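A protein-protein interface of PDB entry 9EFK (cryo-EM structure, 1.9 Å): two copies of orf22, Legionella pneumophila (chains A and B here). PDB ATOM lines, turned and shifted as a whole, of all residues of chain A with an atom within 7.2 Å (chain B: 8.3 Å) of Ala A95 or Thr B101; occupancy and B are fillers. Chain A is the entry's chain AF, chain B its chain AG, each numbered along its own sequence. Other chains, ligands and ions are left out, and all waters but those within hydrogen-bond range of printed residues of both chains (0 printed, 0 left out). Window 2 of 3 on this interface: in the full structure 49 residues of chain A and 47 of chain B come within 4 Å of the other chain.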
ATOM      1  N   TYR A  93      -1.134 -14.385  32.206  1.00  0.00           N
ATOM      2  CA  TYR A  93      -0.621 -15.421  33.082  1.00  0.00           C
ATOM      3  C   TYR A  93       0.902 -15.441  33.054  1.00  0.00           C
ATOM      4  O   TYR A  93       1.542 -14.892  32.155  1.00  0.00           O
ATOM      5  CB  TYR A  93      -1.159 -16.788  32.672  1.00  0.00           C
ATOM      6  CG  TYR A  93      -2.662 -16.862  32.599  1.00  0.00           C
ATOM      7  CD1 TYR A  93      -3.431 -16.839  33.749  1.00  0.00           C
ATOM      8  CD2 TYR A  93      -3.311 -16.963  31.380  1.00  0.00           C
ATOM      9  CE1 TYR A  93      -4.802 -16.904  33.685  1.00  0.00           C
ATOM     10  CE2 TYR A  93      -4.681 -17.030  31.309  1.00  0.00           C
ATOM     11  CZ  TYR A  93      -5.421 -17.005  32.464  1.00  0.00           C
ATOM     12  OH  TYR A  93      -6.789 -17.074  32.399  1.00  0.00           O
ATOM     13  N   SER A  94       1.484 -16.086  34.059  1.00  0.00           N
ATOM     14  CA  SER A  94       2.915 -16.327  34.047  1.00  0.00           C
ATOM     15  C   SER A  94       3.254 -17.393  33.011  1.00  0.00           C
ATOM     16  O   SER A  94       2.384 -18.107  32.515  1.00  0.00           O
ATOM     17  CB  SER A  94       3.397 -16.758  35.428  1.00  0.00           C
ATOM     18  OG  SER A  94       3.079 -15.779  36.394  1.00  0.00           O
ATOM     19  N   ALA A  95       4.542 -17.489  32.680  1.00  0.00           N
ATOM     20  CA  ALA A  95       4.969 -18.437  31.657  1.00  0.00           C
ATOM     21  C   ALA A  95       4.646 -19.870  32.059  1.00  0.00           C
ATOM     22  O   ALA A  95       4.124 -20.648  31.254  1.00  0.00           O
ATOM     23  CB  ALA A  95       6.463 -18.277  31.383  1.00  0.00           C
ATOM     24  N   THR A  96       4.938 -20.239  33.305  1.00  0.00           N
ATOM     25  CA  THR A  96       4.633 -21.574  33.824  1.00  0.00           C
ATOM     26  C   THR A  96       3.821 -21.406  35.103  1.00  0.00           C
ATOM     27  O   THR A  96       4.362 -21.409  36.207  1.00  0.00           O
ATOM     28  CB  THR A  96       5.903 -22.389  34.065  1.00  0.00           C
ATOM     29  OG1 THR A  96       6.867 -21.587  34.754  1.00  0.00           O
ATOM     30  CG2 THR A  96       6.488 -22.865  32.754  1.00  0.00           C
ATOM     31  N   ILE A  97       2.507 -21.277  34.948  1.00  0.00           N
ATOM     32  CA  ILE A  97       1.633 -21.132  36.103  1.00  0.00           C
ATOM     33  C   ILE A  97       1.530 -22.458  36.839  1.00  0.00           C
ATOM     34  O   ILE A  97       1.518 -23.532  36.227  1.00  0.00           O
ATOM     35  CB  ILE A  97       0.245 -20.639  35.664  1.00  0.00           C
ATOM     36  CG1 ILE A  97      -0.276 -21.500  34.516  1.00  0.00           C
ATOM     37  CG2 ILE A  97       0.302 -19.189  35.263  1.00  0.00           C
ATOM     38  CD1 ILE A  97      -1.677 -21.163  34.096  1.00  0.00           C
ATOM     39  N   SER B   2       5.903 -15.603  23.296  1.00  0.00           N
ATOM     40  CA  SER B   2       5.957 -14.320  23.982  1.00  0.00           C
ATOM     41  C   SER B   2       4.740 -14.127  24.877  1.00  0.00           C
ATOM     42  O   SER B   2       3.626 -14.519  24.529  1.00  0.00           O
ATOM     43  CB  SER B   2       6.060 -13.174  22.975  1.00  0.00           C
ATOM     44  OG  SER B   2       4.885 -13.063  22.189  1.00  0.00           O
ATOM     45  N   ASN B   3       4.964 -13.535  26.043  1.00  0.00           N
ATOM     46  CA  ASN B   3       3.902 -13.220  26.987  1.00  0.00           C
ATOM     47  C   ASN B   3       3.831 -11.701  27.089  1.00  0.00           C
ATOM     48  O   ASN B   3       4.406 -11.089  27.986  1.00  0.00           O
ATOM     49  CB  ASN B   3       4.170 -13.873  28.345  1.00  0.00           C
ATOM     50  CG  ASN B   3       4.349 -15.375  28.246  1.00  0.00           C
ATOM     51  OD1 ASN B   3       3.380 -16.127  28.250  1.00  0.00           O
ATOM     52  ND2 ASN B   3       5.595 -15.818  28.161  1.00  0.00           N
ATOM     53  N   TYR B  93      -5.005 -28.896  21.889  1.00  0.00           N
ATOM     54  CA  TYR B  93      -4.808 -29.510  23.193  1.00  0.00           C
ATOM     55  C   TYR B  93      -5.172 -30.985  23.134  1.00  0.00           C
ATOM     56  O   TYR B  93      -6.162 -31.366  22.503  1.00  0.00           O
ATOM     57  CB  TYR B  93      -5.638 -28.798  24.266  1.00  0.00           C
ATOM     58  CG  TYR B  93      -5.253 -27.350  24.442  1.00  0.00           C
ATOM     59  CD1 TYR B  93      -4.085 -27.000  25.099  1.00  0.00           C
ATOM     60  CD2 TYR B  93      -6.046 -26.336  23.938  1.00  0.00           C
ATOM     61  CE1 TYR B  93      -3.723 -25.682  25.254  1.00  0.00           C
ATOM     62  CE2 TYR B  93      -5.695 -25.017  24.090  1.00  0.00           C
ATOM     63  CZ  TYR B  93      -4.533 -24.694  24.746  1.00  0.00           C
ATOM     64  OH  TYR B  93      -4.184 -23.375  24.895  1.00  0.00           O
ATOM     65  N   SER B  98      -1.803 -34.240  29.643  1.00  0.00           N
ATOM     66  CA  SER B  98      -0.691 -33.615  28.939  1.00  0.00           C
ATOM     67  C   SER B  98      -0.181 -32.460  29.794  1.00  0.00           C
ATOM     68  O   SER B  98      -0.487 -32.360  30.986  1.00  0.00           O
ATOM     69  CB  SER B  98      -1.139 -33.181  27.536  1.00  0.00           C
ATOM     70  OG  SER B  98      -0.027 -32.954  26.692  1.00  0.00           O
ATOM     71  N   ASN B  99       0.618 -31.581  29.201  1.00  0.00           N
ATOM     72  CA  ASN B  99       1.171 -30.429  29.895  1.00  0.00           C
ATOM     73  C   ASN B  99       0.464 -29.155  29.456  1.00  0.00           C
ATOM     74  O   ASN B  99      -0.030 -29.056  28.332  1.00  0.00           O
ATOM     75  CB  ASN B  99       2.671 -30.288  29.635  1.00  0.00           C
ATOM     76  CG  ASN B  99       3.478 -31.386  30.278  1.00  0.00           C
ATOM     77  OD1 ASN B  99       3.127 -31.890  31.339  1.00  0.00           O
ATOM     78  ND2 ASN B  99       4.574 -31.759  29.639  1.00  0.00           N
ATOM     79  N   LEU B 100       0.419 -28.180  30.359  1.00  0.00           N
ATOM     80  CA  LEU B 100      -0.119 -26.864  30.054  1.00  0.00           C
ATOM     81  C   LEU B 100       0.809 -25.802  30.619  1.00  0.00           C
ATOM     82  O   LEU B 100       1.379 -25.978  31.697  1.00  0.00           O
ATOM     83  CB  LEU B 100      -1.527 -26.680  30.625  1.00  0.00           C
ATOM     84  CG  LEU B 100      -2.215 -25.356  30.296  1.00  0.00           C
ATOM     85  CD1 LEU B 100      -2.406 -25.206  28.801  1.00  0.00           C
ATOM     86  CD2 LEU B 100      -3.541 -25.241  31.012  1.00  0.00           C
ATOM     87  N   THR B 101       0.963 -24.706  29.882  1.00  0.00           N
ATOM     88  CA  THR B 101       1.726 -23.558  30.341  1.00  0.00           C
ATOM     89  C   THR B 101       0.888 -22.301  30.175  1.00  0.00           C
ATOM     90  O   THR B 101      -0.045 -22.253  29.373  1.00  0.00           O
ATOM     91  CB  THR B 101       3.046 -23.388  29.578  1.00  0.00           C
ATOM     92  OG1 THR B 101       2.771 -23.059  28.212  1.00  0.00           O
ATOM     93  CG2 THR B 101       3.867 -24.654  29.631  1.00  0.00           C
ATOM     94  N   GLY B 102       1.229 -21.277  30.956  1.00  0.00           N
ATOM     95  CA  GLY B 102       0.604 -19.984  30.763  1.00  0.00           C
ATOM     96  C   GLY B 102       0.958 -19.337  29.444  1.00  0.00           C
ATOM     97  O   GLY B 102       0.202 -18.495  28.957  1.00  0.00           O
ATOM     98  N   SER B 103       2.092 -19.716  28.855  1.00  0.00           N
ATOM     99  CA  SER B 103       2.433 -19.233  27.523  1.00  0.00           C
ATOM    100  C   SER B 103       1.415 -19.701  26.493  1.00  0.00           C
ATOM    101  O   SER B 103       1.064 -18.954  25.575  1.00  0.00           O
ATOM    102  CB  SER B 103       3.836 -19.699  27.139  1.00  0.00           C
ATOM    103  OG  SER B 103       4.805 -19.192  28.034  1.00  0.00           O
ATOM    104  N   ASP B 104       0.933 -20.938  26.626  1.00  0.00           N
ATOM    105  CA  ASP B 104      -0.094 -21.431  25.716  1.00  0.00           C
ATOM    106  C   ASP B 104      -1.370 -20.610  25.831  1.00  0.00           C
ATOM    107  O   ASP B 104      -1.937 -20.179  24.821  1.00  0.00           O
ATOM    108  CB  ASP B 104      -0.390 -22.903  26.001  1.00  0.00           C
ATOM    109  CG  ASP B 104       0.806 -23.796  25.771  1.00  0.00           C
ATOM    110  OD1 ASP B 104       1.556 -23.554  24.805  1.00  0.00           O
ATOM    111  OD2 ASP B 104       0.998 -24.744  26.560  1.00  0.00           O
ATOM    112  N   LEU B 105      -1.836 -20.379  27.060  1.00  0.00           N
ATOM    113  CA  LEU B 105      -3.068 -19.626  27.261  1.00  0.00           C
ATOM    114  C   LEU B 105      -2.925 -18.188  26.791  1.00  0.00           C
ATOM    115  O   LEU B 105      -3.833 -17.642  26.158  1.00  0.00           O
ATOM    116  CB  LEU B 105      -3.475 -19.665  28.731  1.00  0.00           C
ATOM    117  CG  LEU B 105      -3.853 -21.038  29.280  1.00  0.00           C
ATOM    118  CD1 LEU B 105      -4.219 -20.936  30.740  1.00  0.00           C
ATOM    119  CD2 LEU B 105      -4.997 -21.618  28.484  1.00  0.00           C
ATOM    120  N   ASN B 106      -1.791 -17.556  27.098  1.00  0.00           N
ATOM    121  CA  ASN B 106      -1.579 -16.173  26.687  1.00  0.00           C
ATOM    122  C   ASN B 106      -1.607 -16.038  25.174  1.00  0.00           C
ATOM    123  O   ASN B 106      -2.189 -15.088  24.642  1.00  0.00           O
ATOM    124  CB  ASN B 106      -0.256 -15.652  27.240  1.00  0.00           C
ATOM    125  CG  ASN B 106      -0.342 -15.280  28.700  1.00  0.00           C
ATOM    126  OD1 ASN B 106      -1.422 -15.039  29.225  1.00  0.00           O
ATOM    127  ND2 ASN B 106       0.801 -15.221  29.361  1.00  0.00           N
ATOM    128  N   GLY B 107      -0.986 -16.977  24.463  1.00  0.00           N
ATOM    129  CA  GLY B 107      -0.982 -16.908  23.012  1.00  0.00           C
ATOM    130  C   GLY B 107      -2.373 -17.008  22.420  1.00  0.00           C
ATOM    131  O   GLY B 107      -2.694 -16.322  21.450  1.00  0.00           O
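Thr B101 touches just one residue of chain A: Ala A95 (3.4 Å).
Printed residues of chain A within 4 Å of Leu B105: Tyr A93.
Printed residues of chain B within 4 Å of Ser A94: Gly B102 (3.1 Å).
Of the printed residues of chain A, Gly B102 touches Ser A94 (3.1 Å), Ala A95 (3.0 Å) and Ile A97 (3.9 Å).
Printed residues of chain A within 4 Å of Asn B106: Tyr A93.
Of the printed residues of chain A, Ser B103 touches Ala A95 (3.3 Å).
Asn B3 touches none of the printed residues of chain A.
Leu B100 touches none of the printed residues of chain A.
The nearest printed residue of chain A that does not touch Asn B106 is Ser A94 (4.6 Å).
Of the 5 printed residues of chain A, 4 touch a printed residue of chain B.
Hydrophobic or aromatic side chains of chain B within 4 Å of the printed part of chain A: Leu B105.
Along chain B the printed residues that touch a printed residue of chain A span positions 101 to 106.
Among the printed residues, 7 pairs touch across the chains.
Among the printed residues, no Asp or Glu carboxylate lies within 4 Å of a Lys or Arg side-chain nitrogen of the other chain.
Among the printed residues, pairs that only touch across the chains: Ser A94 with Gly B102 (3.1 Å), Ala A95 with Thr B101 (3.4 Å), Tyr A93 with Leu B105 (3.8 Å) and Ile A97 with Gly B102 (3.9 Å).
The backbone carbonyl oxygen (O) of Tyr A93 is in hydrogen-bond range of the side-chain amide nitrogen (ND2) of Asn B106, at 2.9 Å.
N of Gly B102 sits at hydrogen-bond distance from O of Ala A95, at 3.0 Å.
N of Ser B103 lies within hydrogen-bond range of O of Ala A95 (3.3 Å).
OG of Ser B103 sits close to OD1 of Asn B3 (3.4 Å).
The side-chain amide nitrogen (ND2) of Asn B106 is in hydrogen-bond range of the side-chain amide oxygen (OD1) of Asn B3, 3.0 Å away.
The side-chain hydroxyl (OG1) of Thr B101 sits close to the backbone NH (N) of Ser B103, 3.5 Å away.
The side-chain carboxylate of Asp B104 sits at hydrogen-bond distance from the side-chain hydroxyl of Thr B101 (3.0 Å).
ND2 of Asn B106 sits close to O of Gly B102.
1 position is printed for both chains.
Of the 7 pairs that touch across the chains among the printed residues, none has its exchanged pair printed and touching as well.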
